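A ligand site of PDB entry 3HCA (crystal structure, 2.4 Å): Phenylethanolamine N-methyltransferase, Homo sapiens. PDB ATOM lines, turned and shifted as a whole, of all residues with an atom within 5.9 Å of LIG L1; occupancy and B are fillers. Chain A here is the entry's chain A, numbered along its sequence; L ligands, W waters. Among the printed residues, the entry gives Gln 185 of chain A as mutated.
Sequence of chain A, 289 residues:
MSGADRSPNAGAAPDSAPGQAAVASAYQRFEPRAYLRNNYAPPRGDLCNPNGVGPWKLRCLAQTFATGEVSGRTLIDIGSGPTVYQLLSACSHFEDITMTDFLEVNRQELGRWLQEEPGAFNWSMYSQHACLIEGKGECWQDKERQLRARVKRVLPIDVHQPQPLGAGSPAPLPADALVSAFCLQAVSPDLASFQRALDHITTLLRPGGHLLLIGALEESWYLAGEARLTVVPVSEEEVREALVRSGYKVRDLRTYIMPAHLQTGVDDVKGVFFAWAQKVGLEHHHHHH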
ATOM      1  N   TYR A  35      26.771  -0.155  32.571  1.00  0.00           N
ATOM      2  CA  TYR A  35      26.221  -0.391  31.240  1.00  0.00           C
ATOM      3  C   TYR A  35      25.012  -1.308  31.298  1.00  0.00           C
ATOM      4  O   TYR A  35      23.990  -1.052  30.655  1.00  0.00           O
ATOM      5  CB  TYR A  35      27.286  -0.958  30.307  1.00  0.00           C
ATOM      6  CG  TYR A  35      26.739  -1.327  28.941  1.00  0.00           C
ATOM      7  CD1 TYR A  35      26.495  -0.350  27.984  1.00  0.00           C
ATOM      8  CD2 TYR A  35      26.466  -2.650  28.616  1.00  0.00           C
ATOM      9  CE1 TYR A  35      25.991  -0.681  26.736  1.00  0.00           C
ATOM     10  CE2 TYR A  35      25.969  -2.989  27.368  1.00  0.00           C
ATOM     11  CZ  TYR A  35      25.735  -2.001  26.437  1.00  0.00           C
ATOM     12  OH  TYR A  35      25.235  -2.328  25.197  1.00  0.00           O
ATOM     13  N   ASN A  39      20.986  -0.335  30.479  1.00  0.00           N
ATOM     14  CA  ASN A  39      20.403  -0.875  29.262  1.00  0.00           C
ATOM     15  C   ASN A  39      19.634  -2.187  29.406  1.00  0.00           C
ATOM     16  O   ASN A  39      18.840  -2.539  28.536  1.00  0.00           O
ATOM     17  CB  ASN A  39      21.477  -1.016  28.193  1.00  0.00           C
ATOM     18  CG  ASN A  39      22.052   0.312  27.782  1.00  0.00           C
ATOM     19  OD1 ASN A  39      21.331   1.172  27.286  1.00  0.00           O
ATOM     20  ND2 ASN A  39      23.356   0.498  28.001  1.00  0.00           N
ATOM     21  N   TYR A  40      19.877  -2.899  30.500  1.00  0.00           N
ATOM     22  CA  TYR A  40      19.281  -4.219  30.672  1.00  0.00           C
ATOM     23  C   TYR A  40      18.606  -4.405  32.021  1.00  0.00           C
ATOM     24  O   TYR A  40      18.311  -5.521  32.438  1.00  0.00           O
ATOM     25  CB  TYR A  40      20.305  -5.305  30.371  1.00  0.00           C
ATOM     26  CG  TYR A  40      20.791  -5.208  28.950  1.00  0.00           C
ATOM     27  CD1 TYR A  40      21.936  -4.492  28.634  1.00  0.00           C
ATOM     28  CD2 TYR A  40      20.063  -5.774  27.906  1.00  0.00           C
ATOM     29  CE1 TYR A  40      22.365  -4.377  27.333  1.00  0.00           C
ATOM     30  CE2 TYR A  40      20.488  -5.663  26.596  1.00  0.00           C
ATOM     31  CZ  TYR A  40      21.643  -4.961  26.318  1.00  0.00           C
ATOM     32  OH  TYR A  40      22.065  -4.852  25.021  1.00  0.00           O
ATOM     33  N   ARG A  44      14.121  -0.330  30.369  1.00  0.00           N
ATOM     34  CA  ARG A  44      14.517  -1.050  29.163  1.00  0.00           C
ATOM     35  C   ARG A  44      14.646  -2.534  29.414  1.00  0.00           C
ATOM     36  O   ARG A  44      14.494  -3.346  28.498  1.00  0.00           O
ATOM     37  CB  ARG A  44      15.826  -0.499  28.600  1.00  0.00           C
ATOM     38  CG  ARG A  44      15.710   0.895  28.035  1.00  0.00           C
ATOM     39  CD  ARG A  44      17.025   1.411  27.462  1.00  0.00           C
ATOM     40  NE  ARG A  44      16.857   2.749  26.907  1.00  0.00           N
ATOM     41  CZ  ARG A  44      17.806   3.404  26.242  1.00  0.00           C
ATOM     42  NH1 ARG A  44      19.000   2.859  26.063  1.00  0.00           N
ATOM     43  NH2 ARG A  44      17.555   4.628  25.771  1.00  0.00           N
ATOM     44  N   VAL A  53      11.904  -2.657  23.856  1.00  0.00           N
ATOM     45  CA  VAL A  53      13.070  -2.919  23.003  1.00  0.00           C
ATOM     46  C   VAL A  53      13.655  -4.303  23.263  1.00  0.00           C
ATOM     47  O   VAL A  53      14.188  -4.940  22.349  1.00  0.00           O
ATOM     48  CB  VAL A  53      14.163  -1.858  23.216  1.00  0.00           C
ATOM     49  CG1 VAL A  53      14.679  -1.890  24.657  1.00  0.00           C
ATOM     50  CG2 VAL A  53      15.299  -2.055  22.230  1.00  0.00           C
ATOM     51  N   LYS A  57      14.120  -7.151  20.303  1.00  0.00           N
ATOM     52  CA  LYS A  57      15.437  -7.668  19.924  1.00  0.00           C
ATOM     53  C   LYS A  57      15.460  -9.188  19.953  1.00  0.00           C
ATOM     54  O   LYS A  57      16.032  -9.827  19.071  1.00  0.00           O
ATOM     55  CB  LYS A  57      16.525  -7.113  20.831  1.00  0.00           C
ATOM     56  CG  LYS A  57      16.786  -5.632  20.649  1.00  0.00           C
ATOM     57  CD  LYS A  57      18.053  -5.197  21.376  1.00  0.00           C
ATOM     58  CE  LYS A  57      17.928  -5.359  22.882  1.00  0.00           C
ATOM     59  NZ  LYS A  57      19.073  -4.725  23.592  1.00  0.00           N
ATOM     60  N   PHE A 182      25.325  -3.824  19.035  1.00  0.00           N
ATOM     61  CA  PHE A 182      25.750  -2.575  19.648  1.00  0.00           C
ATOM     62  C   PHE A 182      27.262  -2.496  19.799  1.00  0.00           C
ATOM     63  O   PHE A 182      27.776  -2.087  20.845  1.00  0.00           O
ATOM     64  CB  PHE A 182      25.059  -2.393  21.002  1.00  0.00           C
ATOM     65  CG  PHE A 182      23.561  -2.439  20.925  1.00  0.00           C
ATOM     66  CD1 PHE A 182      22.865  -3.548  21.379  1.00  0.00           C
ATOM     67  CD2 PHE A 182      22.849  -1.378  20.393  1.00  0.00           C
ATOM     68  CE1 PHE A 182      21.483  -3.599  21.316  1.00  0.00           C
ATOM     69  CE2 PHE A 182      21.464  -1.419  20.315  1.00  0.00           C
ATOM     70  CZ  PHE A 182      20.778  -2.532  20.779  1.00  0.00           C
ATOM     71  N   GLN A 185      29.012   0.363  15.403  1.00  0.00           N
ATOM     72  CA  GLN A 185      28.601   1.752  15.503  1.00  0.00           C
ATOM     73  C   GLN A 185      29.045   2.358  16.838  1.00  0.00           C
ATOM     74  O   GLN A 185      29.379   3.547  16.909  1.00  0.00           O
ATOM     75  CB  GLN A 185      27.075   1.868  15.318  1.00  0.00           C
ATOM     76  CG  GLN A 185      26.514   3.272  15.528  1.00  0.00           C
ATOM     77  CD  GLN A 185      26.194   3.545  16.986  1.00  0.00           C
ATOM     78  OE1 GLN A 185      26.080   2.614  17.783  1.00  0.00           O
ATOM     79  NE2 GLN A 185      26.052   4.821  17.333  1.00  0.00           N
ATOM     80  N   ALA A 186      29.069   1.532  17.872  1.00  0.00           N
ATOM     81  CA  ALA A 186      29.415   1.990  19.219  1.00  0.00           C
ATOM     82  C   ALA A 186      30.903   2.199  19.413  1.00  0.00           C
ATOM     83  O   ALA A 186      31.334   2.733  20.437  1.00  0.00           O
ATOM     84  CB  ALA A 186      28.862   1.016  20.266  1.00  0.00           C
ATOM     85  N   ALA A 216      22.398   0.693  17.342  1.00  0.00           N
ATOM     86  CA  ALA A 216      21.627   1.889  17.646  1.00  0.00           C
ATOM     87  C   ALA A 216      21.446   2.771  16.416  1.00  0.00           C
ATOM     88  O   ALA A 216      22.383   2.940  15.623  1.00  0.00           O
ATOM     89  CB  ALA A 216      22.293   2.661  18.761  1.00  0.00           C
ATOM     90  N   GLU A 219      22.142   7.471  17.057  1.00  0.00           N
ATOM     91  CA  GLU A 219      22.673   7.729  18.385  1.00  0.00           C
ATOM     92  C   GLU A 219      24.051   8.362  18.259  1.00  0.00           C
ATOM     93  O   GLU A 219      24.844   7.967  17.415  1.00  0.00           O
ATOM     94  CB  GLU A 219      22.777   6.431  19.192  1.00  0.00           C
ATOM     95  CG  GLU A 219      23.561   6.559  20.490  1.00  0.00           C
ATOM     96  CD  GLU A 219      23.705   5.233  21.224  1.00  0.00           C
ATOM     97  OE1 GLU A 219      22.752   4.815  21.913  1.00  0.00           O
ATOM     98  OE2 GLU A 219      24.793   4.618  21.106  1.00  0.00           O
ATOM     99  N   TRP A 221      25.828   9.393  21.371  1.00  0.00           N
ATOM    100  CA  TRP A 221      26.536   9.133  22.617  1.00  0.00           C
ATOM    101  C   TRP A 221      25.745   8.205  23.528  1.00  0.00           C
ATOM    102  O   TRP A 221      24.522   8.114  23.421  1.00  0.00           O
ATOM    103  CB  TRP A 221      26.815  10.443  23.353  1.00  0.00           C
ATOM    104  CG  TRP A 221      25.575  11.172  23.760  1.00  0.00           C
ATOM    105  CD1 TRP A 221      24.904  12.101  23.027  1.00  0.00           C
ATOM    106  CD2 TRP A 221      24.859  11.030  25.000  1.00  0.00           C
ATOM    107  NE1 TRP A 221      23.807  12.550  23.734  1.00  0.00           N
ATOM    108  CE2 TRP A 221      23.762  11.909  24.946  1.00  0.00           C
ATOM    109  CE3 TRP A 221      25.043  10.246  26.138  1.00  0.00           C
ATOM    110  CZ2 TRP A 221      22.847  12.024  25.986  1.00  0.00           C
ATOM    111  CZ3 TRP A 221      24.142  10.359  27.175  1.00  0.00           C
ATOM    112  CH2 TRP A 221      23.052  11.241  27.093  1.00  0.00           C
ATOM    113  N   TYR A 222      26.457   7.528  24.423  1.00  0.00           N
ATOM    114  CA  TYR A 222      25.819   6.746  25.477  1.00  0.00           C
ATOM    115  C   TYR A 222      26.768   6.605  26.657  1.00  0.00           C
ATOM    116  O   TYR A 222      27.993   6.614  26.485  1.00  0.00           O
ATOM    117  CB  TYR A 222      25.363   5.376  24.953  1.00  0.00           C
ATOM    118  CG  TYR A 222      26.457   4.344  24.844  1.00  0.00           C
ATOM    119  CD1 TYR A 222      26.713   3.465  25.881  1.00  0.00           C
ATOM    120  CD2 TYR A 222      27.233   4.243  23.689  1.00  0.00           C
ATOM    121  CE1 TYR A 222      27.713   2.513  25.786  1.00  0.00           C
ATOM    122  CE2 TYR A 222      28.239   3.296  23.589  1.00  0.00           C
ATOM    123  CZ  TYR A 222      28.472   2.426  24.642  1.00  0.00           C
ATOM    124  OH  TYR A 222      29.464   1.468  24.552  1.00  0.00           O
ATOM    125  N   MET A 258      12.397   3.912  19.170  1.00  0.00           N
ATOM    126  CA  MET A 258      12.451   3.963  20.627  1.00  0.00           C
ATOM    127  C   MET A 258      11.316   4.813  21.205  1.00  0.00           C
ATOM    128  O   MET A 258      11.216   6.002  20.923  1.00  0.00           O
ATOM    129  CB  MET A 258      13.816   4.491  21.088  1.00  0.00           C
ATOM    130  CG  MET A 258      14.133   4.266  22.553  1.00  0.00           C
ATOM    131  SD  MET A 258      14.287   2.523  23.003  1.00  0.00           S
ATOM    132  CE  MET A 258      15.745   2.042  22.099  1.00  0.00           C
ATOM    133  N   VAL A 266      20.406   7.895  29.487  1.00  0.00           N
ATOM    134  CA  VAL A 266      21.650   7.131  29.444  1.00  0.00           C
ATOM    135  C   VAL A 266      22.246   7.218  28.043  1.00  0.00           C
ATOM    136  O   VAL A 266      23.348   6.733  27.803  1.00  0.00           O
ATOM    137  CB  VAL A 266      21.445   5.638  29.807  1.00  0.00           C
ATOM    138  CG1 VAL A 266      20.915   5.503  31.228  1.00  0.00           C
ATOM    139  CG2 VAL A 266      20.504   4.975  28.809  1.00  0.00           C
ATOM    140  N   ASP A 267      21.501   7.827  27.133  1.00  0.00           N
ATOM    141  CA  ASP A 267      21.949   8.015  25.755  1.00  0.00           C
ATOM    142  C   ASP A 267      20.929   8.826  24.980  1.00  0.00           C
ATOM    143  O   ASP A 267      19.947   9.291  25.542  1.00  0.00           O
ATOM    144  CB  ASP A 267      22.172   6.651  25.067  1.00  0.00           C
ATOM    145  CG  ASP A 267      20.902   5.798  24.993  1.00  0.00           C
ATOM    146  OD1 ASP A 267      19.792   6.358  24.784  1.00  0.00           O
ATOM    147  OD2 ASP A 267      21.009   4.559  25.132  1.00  0.00           O
ATOM    148  N   VAL A 269      19.724   7.560  21.783  1.00  0.00           N
ATOM    149  CA  VAL A 269      19.301   6.646  20.729  1.00  0.00           C
ATOM    150  C   VAL A 269      17.857   6.938  20.304  1.00  0.00           C
ATOM    151  O   VAL A 269      16.997   7.157  21.150  1.00  0.00           O
ATOM    152  CB  VAL A 269      19.425   5.170  21.199  1.00  0.00           C
ATOM    153  CG1 VAL A 269      18.533   4.913  22.398  1.00  0.00           C
ATOM    154  CG2 VAL A 269      19.097   4.211  20.069  1.00  0.00           C
ATOM    155  N   VAL A 272      16.457   1.293  17.046  1.00  0.00           N
ATOM    156  CA  VAL A 272      17.378   0.160  16.992  1.00  0.00           C
ATOM    157  C   VAL A 272      17.143  -0.607  15.693  1.00  0.00           C
ATOM    158  O   VAL A 272      15.999  -0.859  15.325  1.00  0.00           O
ATOM    159  CB  VAL A 272      17.164  -0.800  18.179  1.00  0.00           C
ATOM    160  CG1 VAL A 272      17.929  -2.085  17.953  1.00  0.00           C
ATOM    161  CG2 VAL A 272      17.579  -0.141  19.491  1.00  0.00           C
HETATM  162  C1  LIG L   1      22.052  -0.303  23.926  1.00  0.00           C
HETATM  163  C2  LIG L   1      20.907  -1.030  24.270  1.00  0.00           C
HETATM  164  C3  LIG L   1      19.646  -0.449  24.098  1.00  0.00           C
HETATM  165  O1  LIG L   1      18.485  -1.149  24.448  1.00  0.00           O
HETATM  166  C4  LIG L   1      19.527   0.842  23.580  1.00  0.00           C
HETATM  167  C5  LIG L   1      20.669   1.552  23.234  1.00  0.00           C
HETATM  168  C6  LIG L   1      21.923   0.979  23.404  1.00  0.00           C
HETATM  169  C7  LIG L   1      23.168   1.783  22.998  1.00  0.00           C
HETATM  170  O2  LIG L   1      23.316   2.921  23.794  1.00  0.00           O
HETATM  171  C8  LIG L   1      24.408   0.913  23.098  1.00  0.00           C
HETATM  172  N1  LIG L   1      25.464   1.573  22.365  1.00  0.00           N
HETATM  173  N1  LG2 L   2      27.073  -6.457  22.724  1.00  0.00           N
HETATM  174  C1  LG2 L   2      26.551  -5.957  23.985  1.00  0.00           C
HETATM  175  C2  LG2 L   2      27.472  -4.892  24.603  1.00  0.00           C
HETATM  176  C3  LG2 L   2      27.910  -3.827  23.594  1.00  0.00           C
HETATM  177  S1  LG2 L   2      28.833  -2.511  24.436  1.00  0.00           S
HETATM  178  C4  LG2 L   2      25.136  -5.417  23.800  1.00  0.00           C
HETATM  179  O1  LG2 L   2      24.734  -4.738  24.678  1.00  0.00           O
HETATM  180  O2  LG2 L   2      24.334  -6.098  22.871  1.00  0.00           O
HETATM  181  C5  LG2 L   2      30.173  -2.214  23.253  1.00  0.00           C
HETATM  182  C6  LG2 L   2      31.413  -3.072  23.463  1.00  0.00           C
HETATM  183  O3  LG2 L   2      32.355  -2.745  22.505  1.00  0.00           O
HETATM  184  C7  LG2 L   2      32.068  -2.772  24.806  1.00  0.00           C
HETATM  185  O4  LG2 L   2      32.055  -3.934  25.597  1.00  0.00           O
HETATM  186  C8  LG2 L   2      33.358  -2.397  24.469  1.00  0.00           C
HETATM  187  O5  LG2 L   2      34.298  -2.890  25.390  1.00  0.00           O
HETATM  188  C9  LG2 L   2      33.566  -2.932  23.160  1.00  0.00           C
HETATM  189  N2  LG2 L   2      34.667  -2.341  22.417  1.00  0.00           N
HETATM  190  C10 LG2 L   2      35.243  -1.163  22.665  1.00  0.00           C
HETATM  191  N3  LG2 L   2      36.235  -0.991  21.711  1.00  0.00           N
HETATM  192  C11 LG2 L   2      36.242  -2.080  20.879  1.00  0.00           C
HETATM  193  C12 LG2 L   2      37.011  -2.418  19.785  1.00  0.00           C
HETATM  194  N4  LG2 L   2      38.055  -1.513  19.332  1.00  0.00           N
HETATM  195  N5  LG2 L   2      36.795  -3.583  19.146  1.00  0.00           N
HETATM  196  C13 LG2 L   2      35.816  -4.407  19.596  1.00  0.00           C
HETATM  197  N6  LG2 L   2      35.064  -4.070  20.672  1.00  0.00           N
HETATM  198  C14 LG2 L   2      35.283  -2.916  21.303  1.00  0.00           C
HETATM  199  O   HOH W   1      27.221  -0.314  22.878  1.00  0.00           O
HETATM  200  O   HOH W   2      17.957  -3.350  25.894  1.00  0.00           O
HETATM  201  O   HOH W   3      22.894   3.129  26.275  1.00  0.00           O
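Water W3 lies within hydrogen-bond range of an oxygen (O2) of LIG L1 (2.5 Å), the side-chain carboxylate (OD2) of Asp 267 (2.6 Å) and the side-chain amide oxygen (OD1) of Asn 39 (2.7 Å). Water W1 lies within hydrogen-bond range of a nitrogen (N1) of LIG L1 (2.6 Å), the backbone carbonyl oxygen (O) of Phe 182 (2.8 Å), a sulfur (S1) of LG2 L2 (3.1 Å) and the side-chain hydroxyl (OH) of Tyr 222 (3.3 Å). Water W2 lies within hydrogen-bond range of an oxygen (O1) of LIG L1 (2.7 Å), the backbone carbonyl oxygen of Asn 39 (2.9 Å) and the side-chain amino group of Lys 57 (2.9 Å).
The side-chain amide nitrogen (ND2) of Asn 39 sits at hydrogen-bond distance from the backbone carbonyl oxygen (O) of Tyr 35. OD2 of Asp 267 is in salt-bridge range of NH1 of Arg 44, 2.8 Å away. NZ of Lys 57 is in hydrogen-bond range of OH of Tyr 40. The backbone NH (N) of Val 269 lies close to the side-chain carboxylate (OD1) of Asp 267, at 3.2 Å. The side-chain amide nitrogen of Gln 185 sits at hydrogen-bond distance from the backbone carbonyl oxygen of Glu 219. The side-chain amide oxygen of Asn 39 is in hydrogen-bond range of the guanidinium group of Arg 44, at 3.1 Å.
Residues that only touch LIG L1: Arg 44 (3.2 Å), Tyr 222 (3.4 Å), Lys 57 (3.7 Å), Asn 39 (3.7 Å), Phe 182 (3.8 Å), Val 53 (3.9 Å) and Tyr 35 (3.9 Å).
O1 of LG2 L2 sits at hydrogen-bond distance from OH of Tyr 40, at 2.7 Å. OE2 of Glu 219 is in salt-bridge range of N1 of LIG L1, 3.4 Å away. An oxygen (O2) of LIG L1 sits at hydrogen-bond distance from the side-chain carboxylate (OD2) of Asp 267, 3.1 Å away. OH of Tyr 35 lies within hydrogen-bond range of O1 of LG2 L2 (2.5 Å).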
